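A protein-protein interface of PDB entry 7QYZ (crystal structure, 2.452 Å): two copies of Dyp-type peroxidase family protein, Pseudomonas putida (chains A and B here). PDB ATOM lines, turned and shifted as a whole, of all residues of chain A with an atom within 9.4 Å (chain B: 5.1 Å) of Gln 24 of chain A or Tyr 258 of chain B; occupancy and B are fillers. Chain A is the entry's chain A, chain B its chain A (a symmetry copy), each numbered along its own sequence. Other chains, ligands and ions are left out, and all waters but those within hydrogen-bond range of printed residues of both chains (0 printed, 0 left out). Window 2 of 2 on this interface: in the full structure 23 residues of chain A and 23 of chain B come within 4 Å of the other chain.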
ATOM      1  N   PHE A  21       2.729  -3.344  -9.159  1.00  0.00           N
ATOM      2  CA  PHE A  21       3.842  -2.450  -8.885  1.00  0.00           C
ATOM      3  C   PHE A  21       4.698  -2.984  -7.748  1.00  0.00           C
ATOM      4  O   PHE A  21       4.199  -3.608  -6.807  1.00  0.00           O
ATOM      5  CB  PHE A  21       3.347  -1.046  -8.532  1.00  0.00           C
ATOM      6  CG  PHE A  21       2.639  -0.359  -9.657  1.00  0.00           C
ATOM      7  CD1 PHE A  21       1.293  -0.591  -9.888  1.00  0.00           C
ATOM      8  CD2 PHE A  21       3.318   0.516 -10.489  1.00  0.00           C
ATOM      9  CE1 PHE A  21       0.636   0.037 -10.927  1.00  0.00           C
ATOM     10  CE2 PHE A  21       2.668   1.148 -11.531  1.00  0.00           C
ATOM     11  CZ  PHE A  21       1.323   0.909 -11.750  1.00  0.00           C
ATOM     12  N   THR A  22       5.997  -2.726  -7.847  1.00  0.00           N
ATOM     13  CA  THR A  22       6.957  -3.040  -6.799  1.00  0.00           C
ATOM     14  C   THR A  22       7.401  -1.744  -6.137  1.00  0.00           C
ATOM     15  O   THR A  22       7.773  -0.788  -6.825  1.00  0.00           O
ATOM     16  CB  THR A  22       8.167  -3.789  -7.367  1.00  0.00           C
ATOM     17  OG1 THR A  22       7.733  -5.017  -7.963  1.00  0.00           O
ATOM     18  CG2 THR A  22       9.177  -4.093  -6.266  1.00  0.00           C
ATOM     19  N   LEU A  23       7.349  -1.709  -4.808  1.00  0.00           N
ATOM     20  CA  LEU A  23       7.793  -0.540  -4.056  1.00  0.00           C
ATOM     21  C   LEU A  23       9.312  -0.585  -3.933  1.00  0.00           C
ATOM     22  O   LEU A  23       9.861  -1.462  -3.260  1.00  0.00           O
ATOM     23  CB  LEU A  23       7.130  -0.505  -2.681  1.00  0.00           C
ATOM     24  CG  LEU A  23       7.461   0.704  -1.803  1.00  0.00           C
ATOM     25  CD1 LEU A  23       6.854   1.972  -2.381  1.00  0.00           C
ATOM     26  CD2 LEU A  23       6.986   0.479  -0.377  1.00  0.00           C
ATOM     27  N   GLN A  24       9.994   0.353  -4.588  1.00  0.00           N
ATOM     28  CA  GLN A  24      11.450   0.411  -4.555  1.00  0.00           C
ATOM     29  C   GLN A  24      12.003   1.677  -3.922  1.00  0.00           C
ATOM     30  O   GLN A  24      13.112   1.642  -3.381  1.00  0.00           O
ATOM     31  CB  GLN A  24      12.025   0.268  -5.974  1.00  0.00           C
ATOM     32  CG  GLN A  24      12.003  -1.157  -6.506  1.00  0.00           C
ATOM     33  CD  GLN A  24      12.533  -1.263  -7.923  1.00  0.00           C
ATOM     34  OE1 GLN A  24      12.012  -0.632  -8.842  1.00  0.00           O
ATOM     35  NE2 GLN A  24      13.576  -2.063  -8.106  1.00  0.00           N
ATOM     36  N   SER A  25      11.270   2.790  -3.971  1.00  0.00           N
ATOM     37  CA  SER A  25      11.678   4.045  -3.340  1.00  0.00           C
ATOM     38  C   SER A  25      10.585   4.446  -2.357  1.00  0.00           C
ATOM     39  O   SER A  25       9.681   5.224  -2.701  1.00  0.00           O
ATOM     40  CB  SER A  25      11.920   5.134  -4.382  1.00  0.00           C
ATOM     41  OG  SER A  25      12.438   6.306  -3.779  1.00  0.00           O
ATOM     42  N   PRO A  26      10.629   3.940  -1.121  1.00  0.00           N
ATOM     43  CA  PRO A  26       9.527   4.202  -0.179  1.00  0.00           C
ATOM     44  C   PRO A  26       9.427   5.650   0.266  1.00  0.00           C
ATOM     45  O   PRO A  26       8.348   6.068   0.705  1.00  0.00           O
ATOM     46  CB  PRO A  26       9.851   3.278   1.003  1.00  0.00           C
ATOM     47  CG  PRO A  26      11.333   3.103   0.940  1.00  0.00           C
ATOM     48  CD  PRO A  26      11.686   3.105  -0.522  1.00  0.00           C
ATOM     49  N   GLU A  27      10.507   6.428   0.172  1.00  0.00           N
ATOM     50  CA  GLU A  27      10.453   7.826   0.582  1.00  0.00           C
ATOM     51  C   GLU A  27       9.537   8.654  -0.310  1.00  0.00           C
ATOM     52  O   GLU A  27       9.042   9.697   0.129  1.00  0.00           O
ATOM     53  CB  GLU A  27      11.860   8.431   0.587  1.00  0.00           C
ATOM     54  CG  GLU A  27      12.806   7.837   1.626  1.00  0.00           C
ATOM     55  CD  GLU A  27      13.406   6.508   1.200  1.00  0.00           C
ATOM     56  OE1 GLU A  27      13.260   6.137   0.015  1.00  0.00           O
ATOM     57  OE2 GLU A  27      14.024   5.836   2.051  1.00  0.00           O
ATOM     58  N   ALA A  28       9.301   8.214  -1.544  1.00  0.00           N
ATOM     59  CA  ALA A  28       8.429   8.911  -2.477  1.00  0.00           C
ATOM     60  C   ALA A  28       6.996   8.399  -2.439  1.00  0.00           C
ATOM     61  O   ALA A  28       6.174   8.839  -3.249  1.00  0.00           O
ATOM     62  CB  ALA A  28       8.980   8.793  -3.901  1.00  0.00           C
ATOM     63  N   LEU A  29       6.683   7.480  -1.528  1.00  0.00           N
ATOM     64  CA  LEU A  29       5.333   6.925  -1.474  1.00  0.00           C
ATOM     65  C   LEU A  29       4.262   7.955  -1.128  1.00  0.00           C
ATOM     66  O   LEU A  29       3.191   7.917  -1.760  1.00  0.00           O
ATOM     67  CB  LEU A  29       5.289   5.751  -0.488  1.00  0.00           C
ATOM     68  CG  LEU A  29       3.975   4.968  -0.476  1.00  0.00           C
ATOM     69  CD1 LEU A  29       3.696   4.384  -1.853  1.00  0.00           C
ATOM     70  CD2 LEU A  29       3.995   3.876   0.581  1.00  0.00           C
ATOM     71  N   PRO A  52       3.629  -7.036   0.981  1.00  0.00           N
ATOM     72  CA  PRO A  52       4.858  -6.249   1.192  1.00  0.00           C
ATOM     73  C   PRO A  52       4.604  -4.766   1.405  1.00  0.00           C
ATOM     74  O   PRO A  52       5.402  -4.105   2.081  1.00  0.00           O
ATOM     75  CB  PRO A  52       5.667  -6.508  -0.087  1.00  0.00           C
ATOM     76  CG  PRO A  52       4.663  -6.935  -1.096  1.00  0.00           C
ATOM     77  CD  PRO A  52       3.647  -7.716  -0.328  1.00  0.00           C
ATOM     78  N   LEU A  53       3.518  -4.220   0.851  1.00  0.00           N
ATOM     79  CA  LEU A  53       3.207  -2.811   1.080  1.00  0.00           C
ATOM     80  C   LEU A  53       2.759  -2.573   2.516  1.00  0.00           C
ATOM     81  O   LEU A  53       3.131  -1.565   3.130  1.00  0.00           O
ATOM     82  CB  LEU A  53       2.135  -2.342   0.100  1.00  0.00           C
ATOM     83  CG  LEU A  53       1.595  -0.930   0.332  1.00  0.00           C
ATOM     84  CD1 LEU A  53       2.715   0.098   0.243  1.00  0.00           C
ATOM     85  CD2 LEU A  53       0.491  -0.615  -0.660  1.00  0.00           C
ATOM     86  N   ALA A  56       5.925  -2.962   4.618  1.00  0.00           N
ATOM     87  CA  ALA A  56       6.834  -1.827   4.516  1.00  0.00           C
ATOM     88  C   ALA A  56       6.374  -0.658   5.377  1.00  0.00           C
ATOM     89  O   ALA A  56       7.198   0.159   5.800  1.00  0.00           O
ATOM     90  CB  ALA A  56       6.969  -1.388   3.058  1.00  0.00           C
ATOM     91  N   ALA A  82       3.410  -5.355  -4.440  1.00  0.00           N
ATOM     92  CA  ALA A  82       2.998  -4.438  -3.385  1.00  0.00           C
ATOM     93  C   ALA A  82       1.630  -3.824  -3.662  1.00  0.00           C
ATOM     94  O   ALA A  82       0.834  -3.636  -2.735  1.00  0.00           O
ATOM     95  CB  ALA A  82       4.052  -3.344  -3.205  1.00  0.00           C
ATOM     96  N   LEU A 106       3.063   7.259 -10.452  1.00  0.00           N
ATOM     97  CA  LEU A 106       3.490   6.412  -9.346  1.00  0.00           C
ATOM     98  C   LEU A 106       5.001   6.354  -9.184  1.00  0.00           C
ATOM     99  O   LEU A 106       5.480   5.950  -8.118  1.00  0.00           O
ATOM    100  CB  LEU A 106       2.943   4.991  -9.525  1.00  0.00           C
ATOM    101  CG  LEU A 106       1.606   4.680  -8.847  1.00  0.00           C
ATOM    102  CD1 LEU A 106       0.497   5.605  -9.328  1.00  0.00           C
ATOM    103  CD2 LEU A 106       1.220   3.226  -9.067  1.00  0.00           C
ATOM    104  N   ALA A 107       5.760   6.741 -10.208  1.00  0.00           N
ATOM    105  CA  ALA A 107       7.209   6.790 -10.112  1.00  0.00           C
ATOM    106  C   ALA A 107       7.649   8.020  -9.316  1.00  0.00           C
ATOM    107  O   ALA A 107       6.978   9.056  -9.339  1.00  0.00           O
ATOM    108  CB  ALA A 107       7.830   6.823 -11.505  1.00  0.00           C
ATOM    109  N   PRO A 108       8.786   7.938  -8.603  1.00  0.00           N
ATOM    110  CA  PRO A 108       9.701   6.797  -8.505  1.00  0.00           C
ATOM    111  C   PRO A 108       9.396   5.858  -7.341  1.00  0.00           C
ATOM    112  O   PRO A 108      10.189   4.960  -7.063  1.00  0.00           O
ATOM    113  CB  PRO A 108      11.051   7.473  -8.297  1.00  0.00           C
ATOM    114  CG  PRO A 108      10.706   8.663  -7.461  1.00  0.00           C
ATOM    115  CD  PRO A 108       9.332   9.120  -7.911  1.00  0.00           C
ATOM    116  N   ALA A 109       8.261   6.069  -6.671  1.00  0.00           N
ATOM    117  CA  ALA A 109       7.921   5.247  -5.514  1.00  0.00           C
ATOM    118  C   ALA A 109       7.604   3.813  -5.921  1.00  0.00           C
ATOM    119  O   ALA A 109       8.081   2.862  -5.289  1.00  0.00           O
ATOM    120  CB  ALA A 109       6.739   5.860  -4.765  1.00  0.00           C
ATOM    121  N   LEU A 110       6.808   3.638  -6.972  1.00  0.00           N
ATOM    122  CA  LEU A 110       6.358   2.321  -7.409  1.00  0.00           C
ATOM    123  C   LEU A 110       6.732   2.128  -8.870  1.00  0.00           C
ATOM    124  O   LEU A 110       6.355   2.940  -9.722  1.00  0.00           O
ATOM    125  CB  LEU A 110       4.847   2.174  -7.218  1.00  0.00           C
ATOM    126  CG  LEU A 110       4.345   2.340  -5.784  1.00  0.00           C
ATOM    127  CD1 LEU A 110       2.919   2.855  -5.772  1.00  0.00           C
ATOM    128  CD2 LEU A 110       4.441   1.017  -5.045  1.00  0.00           C
ATOM    129  N   SER A 111       7.462   1.057  -9.159  1.00  0.00           N
ATOM    130  CA  SER A 111       7.810   0.696 -10.526  1.00  0.00           C
ATOM    131  C   SER A 111       6.901  -0.427 -11.010  1.00  0.00           C
ATOM    132  O   SER A 111       6.608  -1.367 -10.266  1.00  0.00           O
ATOM    133  CB  SER A 111       9.276   0.268 -10.623  1.00  0.00           C
ATOM    134  OG  SER A 111       9.560  -0.804  -9.740  1.00  0.00           O
ATOM    135  N   LEU A 112       6.455  -0.320 -12.260  1.00  0.00           N
ATOM    136  CA  LEU A 112       5.564  -1.320 -12.835  1.00  0.00           C
ATOM    137  C   LEU A 112       6.293  -2.654 -12.978  1.00  0.00           C
ATOM    138  O   LEU A 112       7.257  -2.766 -13.744  1.00  0.00           O
ATOM    139  CB  LEU A 112       5.042  -0.836 -14.186  1.00  0.00           C
ATOM    140  CG  LEU A 112       3.968  -1.683 -14.870  1.00  0.00           C
ATOM    141  CD1 LEU A 112       2.741  -1.824 -13.984  1.00  0.00           C
ATOM    142  CD2 LEU A 112       3.592  -1.075 -16.210  1.00  0.00           C
ATOM    143  N   ALA A 113       5.829  -3.663 -12.239  1.00  0.00           N
ATOM    144  CA  ALA A 113       6.399  -5.004 -12.263  1.00  0.00           C
ATOM    145  C   ALA A 113       5.699  -5.947 -13.232  1.00  0.00           C
ATOM    146  O   ALA A 113       6.358  -6.817 -13.812  1.00  0.00           O
ATOM    147  CB  ALA A 113       6.364  -5.621 -10.860  1.00  0.00           C
ATOM    148  N   VAL B  74      10.332  -6.547   0.886  1.00  0.00           N
ATOM    149  CA  VAL B  74      10.880  -6.663  -0.457  1.00  0.00           C
ATOM    150  C   VAL B  74      10.396  -7.970  -1.070  1.00  0.00           C
ATOM    151  O   VAL B  74      10.063  -8.932  -0.372  1.00  0.00           O
ATOM    152  CB  VAL B  74      12.418  -6.588  -0.474  1.00  0.00           C
ATOM    153  CG1 VAL B  74      12.881  -5.223  -0.010  1.00  0.00           C
ATOM    154  CG2 VAL B  74      13.010  -7.678   0.397  1.00  0.00           C
ATOM    155  N   GLU B  75      10.367  -7.994  -2.400  1.00  0.00           N
ATOM    156  CA  GLU B  75       9.755  -9.082  -3.156  1.00  0.00           C
ATOM    157  C   GLU B  75      10.838 -10.044  -3.630  1.00  0.00           C
ATOM    158  O   GLU B  75      11.676  -9.688  -4.463  1.00  0.00           O
ATOM    159  CB  GLU B  75       8.961  -8.529  -4.337  1.00  0.00           C
ATOM    160  CG  GLU B  75       7.913  -7.494  -3.950  1.00  0.00           C
ATOM    161  CD  GLU B  75       7.250  -6.856  -5.157  1.00  0.00           C
ATOM    162  OE1 GLU B  75       7.427  -7.378  -6.278  1.00  0.00           O
ATOM    163  OE2 GLU B  75       6.557  -5.830  -4.988  1.00  0.00           O
ATOM    164  N   ASN B  76      10.816 -11.262  -3.097  1.00  0.00           N
ATOM    165  CA  ASN B  76      11.654 -12.357  -3.584  1.00  0.00           C
ATOM    166  C   ASN B  76      10.733 -13.451  -4.101  1.00  0.00           C
ATOM    167  O   ASN B  76      10.236 -14.274  -3.309  1.00  0.00           O
ATOM    168  CB  ASN B  76      12.571 -12.888  -2.484  1.00  0.00           C
ATOM    169  CG  ASN B  76      13.617 -11.875  -2.061  1.00  0.00           C
ATOM    170  OD1 ASN B  76      14.672 -11.759  -2.684  1.00  0.00           O
ATOM    171  ND2 ASN B  76      13.331 -11.137  -0.996  1.00  0.00           N
ATOM    172  N   TRP B 160      18.042 -11.664 -11.043  1.00  0.00           N
ATOM    173  CA  TRP B 160      17.934 -10.270 -10.640  1.00  0.00           C
ATOM    174  C   TRP B 160      17.972  -9.366 -11.865  1.00  0.00           C
ATOM    175  O   TRP B 160      18.840  -9.520 -12.731  1.00  0.00           O
ATOM    176  CB  TRP B 160      19.065  -9.902  -9.681  1.00  0.00           C
ATOM    177  CG  TRP B 160      18.944 -10.529  -8.329  1.00  0.00           C
ATOM    178  CD1 TRP B 160      19.149 -11.841  -8.010  1.00  0.00           C
ATOM    179  CD2 TRP B 160      18.604  -9.867  -7.106  1.00  0.00           C
ATOM    180  NE1 TRP B 160      18.950 -12.037  -6.665  1.00  0.00           N
ATOM    181  CE2 TRP B 160      18.616 -10.840  -6.088  1.00  0.00           C
ATOM    182  CE3 TRP B 160      18.286  -8.546  -6.774  1.00  0.00           C
ATOM    183  CZ2 TRP B 160      18.322 -10.534  -4.760  1.00  0.00           C
ATOM    184  CZ3 TRP B 160      17.995  -8.244  -5.456  1.00  0.00           C
ATOM    185  CH2 TRP B 160      18.014  -9.234  -4.465  1.00  0.00           C
ATOM    186  N   LEU B 243      19.302 -14.373   2.646  1.00  0.00           N
ATOM    187  CA  LEU B 243      18.196 -13.683   1.993  1.00  0.00           C
ATOM    188  C   LEU B 243      17.240 -13.074   3.012  1.00  0.00           C
ATOM    189  O   LEU B 243      16.725 -11.969   2.802  1.00  0.00           O
ATOM    190  CB  LEU B 243      17.455 -14.644   1.064  1.00  0.00           C
ATOM    191  CG  LEU B 243      16.395 -14.012   0.162  1.00  0.00           C
ATOM    192  CD1 LEU B 243      17.023 -12.952  -0.725  1.00  0.00           C
ATOM    193  CD2 LEU B 243      15.694 -15.072  -0.673  1.00  0.00           C
ATOM    194  N   MET B 246      18.957 -10.023   4.136  1.00  0.00           N
ATOM    195  CA  MET B 246      18.867  -8.958   3.142  1.00  0.00           C
ATOM    196  C   MET B 246      17.460  -8.375   3.080  1.00  0.00           C
ATOM    197  O   MET B 246      17.289  -7.168   2.871  1.00  0.00           O
ATOM    198  CB  MET B 246      19.284  -9.488   1.771  1.00  0.00           C
ATOM    199  CG  MET B 246      20.710 -10.006   1.716  1.00  0.00           C
ATOM    200  SD  MET B 246      21.068 -10.881   0.182  1.00  0.00           S
ATOM    201  CE  MET B 246      20.712  -9.606  -1.024  1.00  0.00           C
ATOM    202  N   SER B 247      16.441  -9.215   3.258  1.00  0.00           N
ATOM    203  CA  SER B 247      15.056  -8.769   3.179  1.00  0.00           C
ATOM    204  C   SER B 247      14.607  -7.993   4.409  1.00  0.00           C
ATOM    205  O   SER B 247      13.479  -7.486   4.422  1.00  0.00           O
ATOM    206  CB  SER B 247      14.135  -9.972   2.969  1.00  0.00           C
ATOM    207  OG  SER B 247      14.530 -10.715   1.829  1.00  0.00           O
ATOM    208  N   ILE B 254      16.941  -3.227   5.392  1.00  0.00           N
ATOM    209  CA  ILE B 254      16.760  -3.828   4.076  1.00  0.00           C
ATOM    210  C   ILE B 254      18.019  -3.600   3.257  1.00  0.00           C
ATOM    211  O   ILE B 254      18.589  -2.501   3.265  1.00  0.00           O
ATOM    212  CB  ILE B 254      15.521  -3.245   3.369  1.00  0.00           C
ATOM    213  CG1 ILE B 254      14.244  -3.663   4.099  1.00  0.00           C
ATOM    214  CG2 ILE B 254      15.473  -3.682   1.914  1.00  0.00           C
ATOM    215  CD1 ILE B 254      12.973  -3.163   3.442  1.00  0.00           C
ATOM    216  N   ASP B 255      18.458  -4.642   2.552  1.00  0.00           N
ATOM    217  CA  ASP B 255      19.646  -4.550   1.712  1.00  0.00           C
ATOM    218  C   ASP B 255      19.496  -3.435   0.683  1.00  0.00           C
ATOM    219  O   ASP B 255      18.402  -3.181   0.170  1.00  0.00           O
ATOM    220  CB  ASP B 255      19.894  -5.891   1.016  1.00  0.00           C
ATOM    221  CG  ASP B 255      21.276  -5.987   0.385  1.00  0.00           C
ATOM    222  OD1 ASP B 255      21.683  -5.053  -0.339  1.00  0.00           O
ATOM    223  OD2 ASP B 255      21.957  -7.010   0.612  1.00  0.00           O
ATOM    224  N   GLY B 256      20.611  -2.767   0.382  1.00  0.00           N
ATOM    225  CA  GLY B 256      20.593  -1.666  -0.565  1.00  0.00           C
ATOM    226  C   GLY B 256      20.437  -2.091  -2.009  1.00  0.00           C
ATOM    227  O   GLY B 256      20.116  -1.251  -2.857  1.00  0.00           O
ATOM    228  N   LEU B 257      20.661  -3.374  -2.310  1.00  0.00           N
ATOM    229  CA  LEU B 257      20.489  -3.855  -3.677  1.00  0.00           C
ATOM    230  C   LEU B 257      19.059  -3.672  -4.163  1.00  0.00           C
ATOM    231  O   LEU B 257      18.835  -3.424  -5.353  1.00  0.00           O
ATOM    232  CB  LEU B 257      20.886  -5.326  -3.778  1.00  0.00           C
ATOM    233  CG  LEU B 257      22.371  -5.675  -3.701  1.00  0.00           C
ATOM    234  CD1 LEU B 257      22.541  -7.176  -3.791  1.00  0.00           C
ATOM    235  CD2 LEU B 257      23.148  -4.980  -4.805  1.00  0.00           C
ATOM    236  N   TYR B 258      18.080  -3.780  -3.262  1.00  0.00           N
ATOM    237  CA  TYR B 258      16.680  -3.664  -3.647  1.00  0.00           C
ATOM    238  C   TYR B 258      16.294  -2.260  -4.089  1.00  0.00           C
ATOM    239  O   TYR B 258      15.137  -2.047  -4.465  1.00  0.00           O
ATOM    240  CB  TYR B 258      15.782  -4.110  -2.492  1.00  0.00           C
ATOM    241  CG  TYR B 258      15.859  -5.594  -2.211  1.00  0.00           C
ATOM    242  CD1 TYR B 258      15.244  -6.511  -3.055  1.00  0.00           C
ATOM    243  CD2 TYR B 258      16.544  -6.080  -1.104  1.00  0.00           C
ATOM    244  CE1 TYR B 258      15.311  -7.870  -2.805  1.00  0.00           C
ATOM    245  CE2 TYR B 258      16.615  -7.437  -0.846  1.00  0.00           C
ATOM    246  CZ  TYR B 258      15.996  -8.328  -1.700  1.00  0.00           C
ATOM    247  OH  TYR B 258      16.062  -9.679  -1.448  1.00  0.00           O
ATOM    248  N   ARG B 259      17.220  -1.301  -4.060  1.00  0.00           N
ATOM    249  CA  ARG B 259      16.893   0.042  -4.518  1.00  0.00           C
ATOM    250  C   ARG B 259      17.061   0.179  -6.027  1.00  0.00           C
ATOM    251  O   ARG B 259      16.405   1.028  -6.643  1.00  0.00           O
ATOM    252  CB  ARG B 259      17.757   1.068  -3.782  1.00  0.00           C
ATOM    253  CG  ARG B 259      17.283   2.501  -3.943  1.00  0.00           C
ATOM    254  CD  ARG B 259      17.788   3.374  -2.807  1.00  0.00           C
ATOM    255  NE  ARG B 259      17.286   2.927  -1.510  1.00  0.00           N
ATOM    256  CZ  ARG B 259      16.184   3.395  -0.931  1.00  0.00           C
ATOM    257  NH1 ARG B 259      15.460   4.329  -1.532  1.00  0.00           N
ATOM    258  NH2 ARG B 259      15.806   2.926   0.250  1.00  0.00           N
ATOM    259  N   PHE B 260      17.923  -0.642  -6.638  1.00  0.00           N
ATOM    260  CA  PHE B 260      18.113  -0.625  -8.083  1.00  0.00           C
ATOM    261  C   PHE B 260      17.935  -1.980  -8.749  1.00  0.00           C
ATOM    262  O   PHE B 260      17.946  -2.038  -9.984  1.00  0.00           O
ATOM    263  CB  PHE B 260      19.508  -0.086  -8.437  1.00  0.00           C
ATOM    264  CG  PHE B 260      20.620  -1.073  -8.209  1.00  0.00           C
ATOM    265  CD1 PHE B 260      21.118  -1.300  -6.934  1.00  0.00           C
ATOM    266  CD2 PHE B 260      21.177  -1.764  -9.272  1.00  0.00           C
ATOM    267  CE1 PHE B 260      22.144  -2.205  -6.727  1.00  0.00           C
ATOM    268  CE2 PHE B 260      22.200  -2.668  -9.069  1.00  0.00           C
ATOM    269  CZ  PHE B 260      22.686  -2.890  -7.796  1.00  0.00           C
ATOM    270  N   SER B 261      17.777  -3.062  -7.991  1.00  0.00           N
ATOM    271  CA  SER B 261      17.632  -4.387  -8.572  1.00  0.00           C
ATOM    272  C   SER B 261      16.603  -5.180  -7.784  1.00  0.00           C
ATOM    273  O   SER B 261      16.432  -4.984  -6.578  1.00  0.00           O
ATOM    274  CB  SER B 261      18.965  -5.143  -8.595  1.00  0.00           C
ATOM    275  OG  SER B 261      18.798  -6.434  -9.153  1.00  0.00           O
ATOM    276  N   ARG B 262      15.917  -6.083  -8.482  1.00  0.00           N
ATOM    277  CA  ARG B 262      14.927  -6.941  -7.865  1.00  0.00           C
ATOM    278  C   ARG B 262      14.964  -8.304  -8.541  1.00  0.00           C
ATOM    279  O   ARG B 262      15.133  -8.389  -9.767  1.00  0.00           O
ATOM    280  CB  ARG B 262      13.516  -6.341  -7.959  1.00  0.00           C
ATOM    281  CG  ARG B 262      13.025  -6.101  -9.375  1.00  0.00           C
ATOM    282  CD  ARG B 262      11.658  -5.441  -9.384  1.00  0.00           C
ATOM    283  NE  ARG B 262      10.971  -5.657 -10.653  1.00  0.00           N
ATOM    284  CZ  ARG B 262      10.136  -6.664 -10.886  1.00  0.00           C
ATOM    285  NH1 ARG B 262       9.881  -7.551  -9.932  1.00  0.00           N
ATOM    286  NH2 ARG B 262       9.553  -6.788 -12.071  1.00  0.00           N
ATOM    287  N   PRO B 263      14.832  -9.383  -7.774  1.00  0.00           N
ATOM    288  CA  PRO B 263      14.815 -10.715  -8.387  1.00  0.00           C
ATOM    289  C   PRO B 263      13.494 -10.979  -9.091  1.00  0.00           C
ATOM    290  O   PRO B 263      12.421 -10.627  -8.595  1.00  0.00           O
ATOM    291  CB  PRO B 263      15.017 -11.658  -7.197  1.00  0.00           C
ATOM    292  CG  PRO B 263      14.483 -10.897  -6.027  1.00  0.00           C
ATOM    293  CD  PRO B 263      14.759  -9.442  -6.303  1.00  0.00           C
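The side-chain carboxylate of Glu 75 of chain B lies within hydrogen-bond range of the side-chain hydroxyl of Thr 22 of chain A (2.9 Å). The side-chain carboxylate (OE1) of Glu 27 of chain A is in salt-bridge range of the guanidinium group (NH1) of Arg 259 of chain B (3.2 Å). The backbone NH (N) of Ala 82 of chain A sits at hydrogen-bond distance from the side-chain carboxylate (OE2) of Glu 75 of chain B, at 3.2 Å.
The backbone NH (N) of Ala 82 of chain A is in hydrogen-bond range of the backbone carbonyl oxygen (O) of Phe 21 of chain A, 3.0 Å away. The backbone carbonyl oxygen of Ser 111 of chain A sits at hydrogen-bond distance from the backbone NH of Thr 22 of chain A, 2.8 Å away. N of Gln 24 of chain A sits at hydrogen-bond distance from O of Ala 109 of chain A (3.2 Å). OE1 of Gln 24 of chain A sits at hydrogen-bond distance from OG of Ser 111 of chain A (2.6 Å). The side-chain amide oxygen (OD1) of Asn 76 of chain B is in hydrogen-bond range of the side-chain hydroxyl (OH) of Tyr 258 of chain B (2.8 Å).
Among the printed residues, merely in contact across the chains: Phe 21 of chain A with Glu 75 of chain B (3.7 Å), Thr 22 of chain A with Arg 262 of chain B (3.9 Å), Gln 24 of chain A with Tyr 258 of chain B (3.8 Å) and Ala 113 of chain A with Arg 262 of chain B (3.6 Å).
Of the printed residues of chain B, Gln 24 of chain A touches Tyr 258. Tyr 258 of chain B touches just one residue of chain A: Gln 24 (3.8 Å). Gly 256 of chain B touches none of the printed residues of chain A. Of the printed residues of chain A, Glu 75 of chain B touches Phe 21, Thr 22 and Ala 82. Of the printed residues of chain B, Ala 113 of chain A touches Arg 262 (3.6 Å). Of the printed residues of chain B, Glu 27 of chain A touches Arg 259. Printed residues of chain B within 4 Å of Ala 82 of chain A: Glu 75. Of the printed residues of chain B, Phe 21 of chain A touches Glu 75 (3.7 Å). The nearest printed residue of chain B that does not touch Gln 24 of chain A is Arg 259 of chain B (4.02 Å). The nearest residue of chain A that does not touch Tyr 258 of chain B is Leu 23 of chain A (5.4 Å). The nearest printed residue of chain B that does not touch Phe 21 of chain A is Arg 262 of chain B (7.2 Å).
Printed residues of chain A that touch a printed residue of chain B: Phe 21, Thr 22, Gln 24, Glu 27, Ala 82 and Ala 113. Along chain A the printed residues that touch a printed residue of chain B span positions 21 to 113. Among the printed residues, Asp or Glu carboxylates within 4 Å of a Lys or Arg side-chain nitrogen of the other chain: Glu 27 of chain A with Arg 259 of chain B.
No position is printed for both chains.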
